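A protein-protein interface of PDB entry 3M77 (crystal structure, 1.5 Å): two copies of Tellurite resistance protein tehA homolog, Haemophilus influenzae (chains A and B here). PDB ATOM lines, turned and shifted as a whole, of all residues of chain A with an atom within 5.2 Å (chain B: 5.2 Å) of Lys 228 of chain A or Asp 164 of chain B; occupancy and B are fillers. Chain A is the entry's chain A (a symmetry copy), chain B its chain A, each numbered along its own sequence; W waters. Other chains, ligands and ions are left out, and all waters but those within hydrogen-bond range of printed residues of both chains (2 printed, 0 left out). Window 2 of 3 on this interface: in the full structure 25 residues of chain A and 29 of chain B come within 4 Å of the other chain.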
ATOM      1  N   VAL A 223      10.632  -0.345 -12.314  1.00  0.00           N
ATOM      2  CA  VAL A 223      11.691  -1.021 -11.622  1.00  0.00           C
ATOM      3  C   VAL A 223      12.818  -0.035 -11.371  1.00  0.00           C
ATOM      4  O   VAL A 223      13.696   0.203 -12.220  1.00  0.00           O
ATOM      5  CB  VAL A 223      12.176  -2.212 -12.435  1.00  0.00           C
ATOM      6  CG1 VAL A 223      13.261  -2.962 -11.697  1.00  0.00           C
ATOM      7  CG2 VAL A 223      10.994  -3.108 -12.690  1.00  0.00           C
ATOM      8  N   ASP A 224      12.819   0.499 -10.174  1.00  0.00           N
ATOM      9  CA  ASP A 224      13.708   1.556  -9.817  1.00  0.00           C
ATOM     10  C   ASP A 224      14.749   1.126  -8.784  1.00  0.00           C
ATOM     11  O   ASP A 224      14.908  -0.059  -8.533  1.00  0.00           O
ATOM     12  CB  ASP A 224      12.851   2.733  -9.333  1.00  0.00           C
ATOM     13  CG  ASP A 224      12.051   2.416  -8.080  1.00  0.00           C
ATOM     14  OD1 ASP A 224      12.196   1.288  -7.512  1.00  0.00           O
ATOM     15  OD2 ASP A 224      11.269   3.323  -7.617  1.00  0.00           O
ATOM     16  N   THR A 225      15.456   2.081  -8.189  1.00  0.00           N
ATOM     17  CA  THR A 225      16.494   1.739  -7.226  1.00  0.00           C
ATOM     18  C   THR A 225      15.954   0.983  -6.017  1.00  0.00           C
ATOM     19  O   THR A 225      16.536  -0.030  -5.586  1.00  0.00           O
ATOM     20  CB  THR A 225      17.268   2.981  -6.804  1.00  0.00           C
ATOM     21  OG1 THR A 225      17.942   3.499  -7.956  1.00  0.00           O
ATOM     22  CG2 THR A 225      18.291   2.680  -5.739  1.00  0.00           C
ATOM     23  N   LEU A 226      14.840   1.465  -5.445  1.00  0.00           N
ATOM     24  CA  LEU A 226      14.227   0.747  -4.330  1.00  0.00           C
ATOM     25  C   LEU A 226      13.906  -0.708  -4.696  1.00  0.00           C
ATOM     26  O   LEU A 226      14.189  -1.625  -3.941  1.00  0.00           O
ATOM     27  CB  LEU A 226      12.967   1.440  -3.840  1.00  0.00           C
ATOM     28  CG  LEU A 226      12.238   0.707  -2.725  1.00  0.00           C
ATOM     29  CD1 LEU A 226      13.101   0.482  -1.496  1.00  0.00           C
ATOM     30  CD2 LEU A 226      10.919   1.451  -2.360  1.00  0.00           C
ATOM     31  N   ALA A 227      13.322  -0.933  -5.862  1.00  0.00           N
ATOM     32  CA  ALA A 227      12.942  -2.294  -6.262  1.00  0.00           C
ATOM     33  C   ALA A 227      14.181  -3.172  -6.346  1.00  0.00           C
ATOM     34  O   ALA A 227      14.159  -4.312  -5.926  1.00  0.00           O
ATOM     35  CB  ALA A 227      12.215  -2.260  -7.552  1.00  0.00           C
ATOM     36  N   LYS A 228      15.263  -2.674  -6.951  1.00  0.00           N
ATOM     37  CA  LYS A 228      16.474  -3.467  -7.090  1.00  0.00           C
ATOM     38  C   LYS A 228      17.084  -3.785  -5.702  1.00  0.00           C
ATOM     39  O   LYS A 228      17.555  -4.901  -5.440  1.00  0.00           O
ATOM     40  CB  LYS A 228      17.464  -2.719  -7.983  1.00  0.00           C
ATOM     41  CG  LYS A 228      16.987  -2.534  -9.422  1.00  0.00           C
ATOM     42  CD  LYS A 228      17.938  -1.600 -10.184  1.00  0.00           C
ATOM     43  CE  LYS A 228      17.257  -1.094 -11.447  1.00  0.00           C
ATOM     44  NZ  LYS A 228      18.148  -0.095 -12.144  1.00  0.00           N
ATOM     45  N   ILE A 229      17.054  -2.799  -4.818  1.00  0.00           N
ATOM     46  CA  ILE A 229      17.584  -2.960  -3.436  1.00  0.00           C
ATOM     47  C   ILE A 229      16.809  -4.071  -2.723  1.00  0.00           C
ATOM     48  O   ILE A 229      17.400  -4.960  -2.087  1.00  0.00           O
ATOM     49  CB  ILE A 229      17.447  -1.631  -2.673  1.00  0.00           C
ATOM     50  CG1 ILE A 229      18.579  -0.680  -3.083  1.00  0.00           C
ATOM     51  CG2 ILE A 229      17.333  -1.854  -1.200  1.00  0.00           C
ATOM     52  CD1 ILE A 229      18.460   0.710  -2.551  1.00  0.00           C
ATOM     53  N   LEU A 230      15.493  -4.054  -2.857  1.00  0.00           N
ATOM     54  CA  LEU A 230      14.673  -5.081  -2.227  1.00  0.00           C
ATOM     55  C   LEU A 230      14.964  -6.464  -2.781  1.00  0.00           C
ATOM     56  O   LEU A 230      15.029  -7.440  -2.046  1.00  0.00           O
ATOM     57  CB  LEU A 230      13.173  -4.748  -2.385  1.00  0.00           C
ATOM     58  CG  LEU A 230      12.717  -3.506  -1.652  1.00  0.00           C
ATOM     59  CD1 LEU A 230      11.379  -3.002  -2.093  1.00  0.00           C
ATOM     60  CD2 LEU A 230      12.678  -3.773  -0.147  1.00  0.00           C
ATOM     61  N   TRP A 231      15.067  -6.564  -4.114  1.00  0.00           N
ATOM     62  CA  TRP A 231      15.385  -7.844  -4.708  1.00  0.00           C
ATOM     63  C   TRP A 231      16.700  -8.376  -4.164  1.00  0.00           C
ATOM     64  O   TRP A 231      16.857  -9.600  -3.939  1.00  0.00           O
ATOM     65  CB  TRP A 231      15.421  -7.763  -6.236  1.00  0.00           C
ATOM     66  CG  TRP A 231      14.421  -8.603  -6.923  1.00  0.00           C
ATOM     67  CD1 TRP A 231      13.196  -8.989  -6.460  1.00  0.00           C
ATOM     68  CD2 TRP A 231      14.547  -9.139  -8.230  1.00  0.00           C
ATOM     69  NE1 TRP A 231      12.574  -9.750  -7.384  1.00  0.00           N
ATOM     70  CE2 TRP A 231      13.397  -9.884  -8.478  1.00  0.00           C
ATOM     71  CE3 TRP A 231      15.551  -9.090  -9.200  1.00  0.00           C
ATOM     72  CZ2 TRP A 231      13.186 -10.552  -9.695  1.00  0.00           C
ATOM     73  CZ3 TRP A 231      15.334  -9.777 -10.408  1.00  0.00           C
ATOM     74  CH2 TRP A 231      14.173 -10.492 -10.613  1.00  0.00           C
ATOM     75  N   GLY A 232      17.689  -7.502  -4.000  1.00  0.00           N
ATOM     76  CA  GLY A 232      19.000  -7.970  -3.545  1.00  0.00           C
ATOM     77  C   GLY A 232      18.930  -8.608  -2.158  1.00  0.00           C
ATOM     78  O   GLY A 232      19.461  -9.711  -1.930  1.00  0.00           O
ATOM     79  N   PHE A 274      10.224  -7.173 -13.313  1.00  0.00           N
ATOM     80  CA  PHE A 274      11.618  -6.949 -13.689  1.00  0.00           C
ATOM     81  C   PHE A 274      11.814  -7.299 -15.180  1.00  0.00           C
ATOM     82  O   PHE A 274      12.410  -6.553 -15.950  1.00  0.00           O
ATOM     83  CB  PHE A 274      12.593  -7.743 -12.824  1.00  0.00           C
ATOM     84  CG  PHE A 274      12.985  -7.045 -11.506  1.00  0.00           C
ATOM     85  CD1 PHE A 274      12.087  -6.933 -10.477  1.00  0.00           C
ATOM     86  CD2 PHE A 274      14.244  -6.523 -11.339  1.00  0.00           C
ATOM     87  CE1 PHE A 274      12.405  -6.304  -9.284  1.00  0.00           C
ATOM     88  CE2 PHE A 274      14.582  -5.876 -10.145  1.00  0.00           C
ATOM     89  CZ  PHE A 274      13.656  -5.768  -9.134  1.00  0.00           C
ATOM     90  N   ASN A 278      12.833  -4.867 -18.464  1.00  0.00           N
ATOM     91  CA  ASN A 278      14.165  -5.179 -18.989  1.00  0.00           C
ATOM     92  C   ASN A 278      15.279  -4.911 -17.970  1.00  0.00           C
ATOM     93  O   ASN A 278      16.331  -4.306 -18.288  1.00  0.00           O
ATOM     94  CB  ASN A 278      14.459  -4.434 -20.277  1.00  0.00           C
ATOM     95  CG  ASN A 278      15.655  -5.023 -21.024  1.00  0.00           C
ATOM     96  OD1 ASN A 278      16.019  -6.181 -20.807  1.00  0.00           O
ATOM     97  ND2 ASN A 278      16.288  -4.216 -21.894  1.00  0.00           N
ATOM     98  N   VAL A 279      15.051  -5.393 -16.761  1.00  0.00           N
ATOM     99  CA  VAL A 279      16.062  -5.338 -15.702  1.00  0.00           C
ATOM    100  C   VAL A 279      16.329  -6.776 -15.263  1.00  0.00           C
ATOM    101  O   VAL A 279      15.426  -7.515 -14.863  1.00  0.00           O
ATOM    102  CB  VAL A 279      15.552  -4.515 -14.478  1.00  0.00           C
ATOM    103  CG1 VAL A 279      16.548  -4.546 -13.376  1.00  0.00           C
ATOM    104  CG2 VAL A 279      15.293  -3.063 -14.906  1.00  0.00           C
ATOM    105  N   LEU A 280      17.577  -7.189 -15.379  1.00  0.00           N
ATOM    106  CA  LEU A 280      17.999  -8.497 -14.921  1.00  0.00           C
ATOM    107  C   LEU A 280      17.044  -9.583 -15.446  1.00  0.00           C
ATOM    108  O   LEU A 280      16.486 -10.408 -14.688  1.00  0.00           O
ATOM    109  CB  LEU A 280      18.123  -8.527 -13.407  1.00  0.00           C
ATOM    110  CG  LEU A 280      19.076  -7.501 -12.787  1.00  0.00           C
ATOM    111  CD1 LEU A 280      18.785  -7.370 -11.288  1.00  0.00           C
ATOM    112  CD2 LEU A 280      20.496  -7.942 -13.075  1.00  0.00           C
ATOM    113  N   TYR B 162      28.468  -3.651 -14.272  1.00  0.00           N
ATOM    114  CA  TYR B 162      27.285  -4.412 -13.879  1.00  0.00           C
ATOM    115  C   TYR B 162      26.466  -3.634 -12.842  1.00  0.00           C
ATOM    116  O   TYR B 162      26.444  -4.000 -11.650  1.00  0.00           O
ATOM    117  CB  TYR B 162      27.667  -5.779 -13.318  1.00  0.00           C
ATOM    118  CG  TYR B 162      28.402  -6.669 -14.294  1.00  0.00           C
ATOM    119  CD1 TYR B 162      27.700  -7.401 -15.235  1.00  0.00           C
ATOM    120  CD2 TYR B 162      29.771  -6.795 -14.257  1.00  0.00           C
ATOM    121  CE1 TYR B 162      28.360  -8.224 -16.146  1.00  0.00           C
ATOM    122  CE2 TYR B 162      30.435  -7.595 -15.155  1.00  0.00           C
ATOM    123  CZ  TYR B 162      29.735  -8.301 -16.093  1.00  0.00           C
ATOM    124  OH  TYR B 162      30.393  -9.118 -17.004  1.00  0.00           O
ATOM    125  N   HIS B 163      25.832  -2.543 -13.259  1.00  0.00           N
ATOM    126  CA  HIS B 163      25.178  -1.663 -12.300  1.00  0.00           C
ATOM    127  C   HIS B 163      23.973  -2.311 -11.631  1.00  0.00           C
ATOM    128  O   HIS B 163      23.799  -2.167 -10.423  1.00  0.00           O
ATOM    129  CB  HIS B 163      24.772  -0.341 -12.920  1.00  0.00           C
ATOM    130  CG  HIS B 163      25.950   0.541 -13.229  1.00  0.00           C
ATOM    131  ND1 HIS B 163      26.794   0.288 -14.291  1.00  0.00           N
ATOM    132  CD2 HIS B 163      26.480   1.596 -12.561  1.00  0.00           C
ATOM    133  CE1 HIS B 163      27.774   1.180 -14.281  1.00  0.00           C
ATOM    134  NE2 HIS B 163      27.598   1.991 -13.254  1.00  0.00           N
ATOM    135  N   ASP B 164      23.123  -2.988 -12.391  1.00  0.00           N
ATOM    136  CA  ASP B 164      21.929  -3.584 -11.773  1.00  0.00           C
ATOM    137  C   ASP B 164      22.290  -4.721 -10.839  1.00  0.00           C
ATOM    138  O   ASP B 164      21.735  -4.816  -9.740  1.00  0.00           O
ATOM    139  CB  ASP B 164      20.923  -4.017 -12.842  1.00  0.00           C
ATOM    140  CG  ASP B 164      20.255  -2.857 -13.503  1.00  0.00           C
ATOM    141  OD1 ASP B 164      20.233  -1.750 -12.937  1.00  0.00           O
ATOM    142  OD2 ASP B 164      19.761  -3.060 -14.622  1.00  0.00           O
ATOM    143  N   LEU B 165      23.236  -5.570 -11.210  1.00  0.00           N
ATOM    144  CA  LEU B 165      23.760  -6.556 -10.267  1.00  0.00           C
ATOM    145  C   LEU B 165      24.362  -5.886  -9.057  1.00  0.00           C
ATOM    146  O   LEU B 165      24.168  -6.340  -7.927  1.00  0.00           O
ATOM    147  CB  LEU B 165      24.820  -7.448 -10.879  1.00  0.00           C
ATOM    148  CG  LEU B 165      24.384  -8.583 -11.780  1.00  0.00           C
ATOM    149  CD1 LEU B 165      25.652  -9.382 -12.170  1.00  0.00           C
ATOM    150  CD2 LEU B 165      23.293  -9.465 -11.127  1.00  0.00           C
ATOM    151  N   GLY B 166      25.090  -4.794  -9.268  1.00  0.00           N
ATOM    152  CA  GLY B 166      25.627  -4.034  -8.149  1.00  0.00           C
ATOM    153  C   GLY B 166      24.537  -3.576  -7.191  1.00  0.00           C
ATOM    154  O   GLY B 166      24.713  -3.641  -5.993  1.00  0.00           O
ATOM    155  N   TYR B 167      23.405  -3.106  -7.710  1.00  0.00           N
ATOM    156  CA  TYR B 167      22.320  -2.672  -6.830  1.00  0.00           C
ATOM    157  C   TYR B 167      21.786  -3.830  -5.984  1.00  0.00           C
ATOM    158  O   TYR B 167      21.339  -3.598  -4.866  1.00  0.00           O
ATOM    159  CB  TYR B 167      21.182  -2.041  -7.621  1.00  0.00           C
ATOM    160  CG  TYR B 167      21.341  -0.568  -7.886  1.00  0.00           C
ATOM    161  CD1 TYR B 167      21.331  -0.075  -9.166  1.00  0.00           C
ATOM    162  CD2 TYR B 167      21.474   0.353  -6.852  1.00  0.00           C
ATOM    163  CE1 TYR B 167      21.443   1.295  -9.416  1.00  0.00           C
ATOM    164  CE2 TYR B 167      21.618   1.730  -7.122  1.00  0.00           C
ATOM    165  CZ  TYR B 167      21.576   2.167  -8.403  1.00  0.00           C
ATOM    166  OH  TYR B 167      21.717   3.534  -8.670  1.00  0.00           O
ATOM    167  N   LEU B 168      21.779  -5.056  -6.529  1.00  0.00           N
ATOM    168  CA  LEU B 168      21.336  -6.227  -5.724  1.00  0.00           C
ATOM    169  C   LEU B 168      22.250  -6.395  -4.504  1.00  0.00           C
ATOM    170  O   LEU B 168      21.787  -6.487  -3.357  1.00  0.00           O
ATOM    171  CB  LEU B 168      21.318  -7.541  -6.489  1.00  0.00           C
ATOM    172  CG  LEU B 168      20.400  -7.673  -7.689  1.00  0.00           C
ATOM    173  CD1 LEU B 168      20.415  -9.065  -8.302  1.00  0.00           C
ATOM    174  CD2 LEU B 168      19.067  -7.361  -7.320  1.00  0.00           C
HETATM  175  O   HOH W   1      19.694  -5.333 -16.159  1.00  0.00           O
HETATM  176  O   HOH W   2      19.780   5.342  -7.512  1.00  0.00           O
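The side-chain carboxylate of Asp 164 of chain B lies within salt-bridge range of the side-chain amino group of Lys 228 of chain A.
O of Phe 274 of chain A lies within hydrogen-bond range of N of Val 279 of chain A.
Thr 225 of chain A touches Tyr 167 of chain B (CG2 to CE2, 3.7 Å). CB of Tyr 167 of chain B touches CB of Lys 228 of chain A (3.8 Å). Lys 228 of chain A touches Leu 168 of chain B (O to CD2, 3.4 Å). CB of Trp 231 of chain A touches CD2 of Leu 168 of chain B, at 3.8 Å. Leu 168 of chain B touches Gly 232 of chain A (O to CA, 3.2 Å). Asp 164 of chain B touches Val 279 of chain A (OD2 to CG1, 3.8 Å). CG of Leu 280 of chain A touches CB of Asp 164 of chain B, at 3.9 Å. Leu 165 of chain B touches Leu 280 of chain A (CD2 to CD2, 3.7 Å). Leu 280 of chain A touches Leu 168 of chain B (CD1 to CD1, 3.8 Å).
Printed residues of chain B within 4 Å of Lys 228 of chain A: Asp 164, Tyr 167 and Leu 168. Of chain A, only Lys 228, Val 279 and Leu 280 come within 4 Å of Asp 164 of chain B. Of the printed residues of chain B, Gly 232 of chain A touches Leu 168. Of the printed residues of chain B, Thr 225 of chain A touches Tyr 167 (3.7 Å). Of the printed residues of chain B, Val 279 of chain A touches Asp 164. Of the printed residues of chain B, Trp 231 of chain A touches Leu 168. Phe 274 of chain A touches none of the printed residues of chain B. Asp 224 of chain A touches none of the printed residues of chain B. The nearest printed residue of chain B that does not touch Lys 228 of chain A is His 163 of chain B (5.9 Å). The nearest printed residue of chain B that does not touch Trp 231 of chain A is Tyr 167 of chain B (6.7 Å).
Of the 7 printed residues of chain B, 4 touch a printed residue of chain A. Hydrophobic or aromatic side chains of chain B that line the printed part of chain A: Leu 165, Tyr 167 and Leu 168. Hydrophobic or aromatic side chains of chain A within 4 Å of the printed part of chain B: Trp 231, Val 279 and Leu 280. Among the printed residues, 10 pairs touch across the chains. Among the printed residues, Asp or Glu carboxylates within 4 Å of a Lys or Arg side-chain nitrogen of the other chain: Lys 228 of chain A with Asp 164 of chain B (2.8 Å).
No position is printed for both chains.
Water W2 bridges the side-chain hydroxyl (OG1) of Thr 225 of chain A and the side-chain hydroxyl (OH) of Tyr 167 of chain B. Water W1 lies within hydrogen-bond range of the side-chain carboxylate of Asp 164 of chain B (2.7 Å) and the backbone NH of Leu 280 of chain A (2.9 Å).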
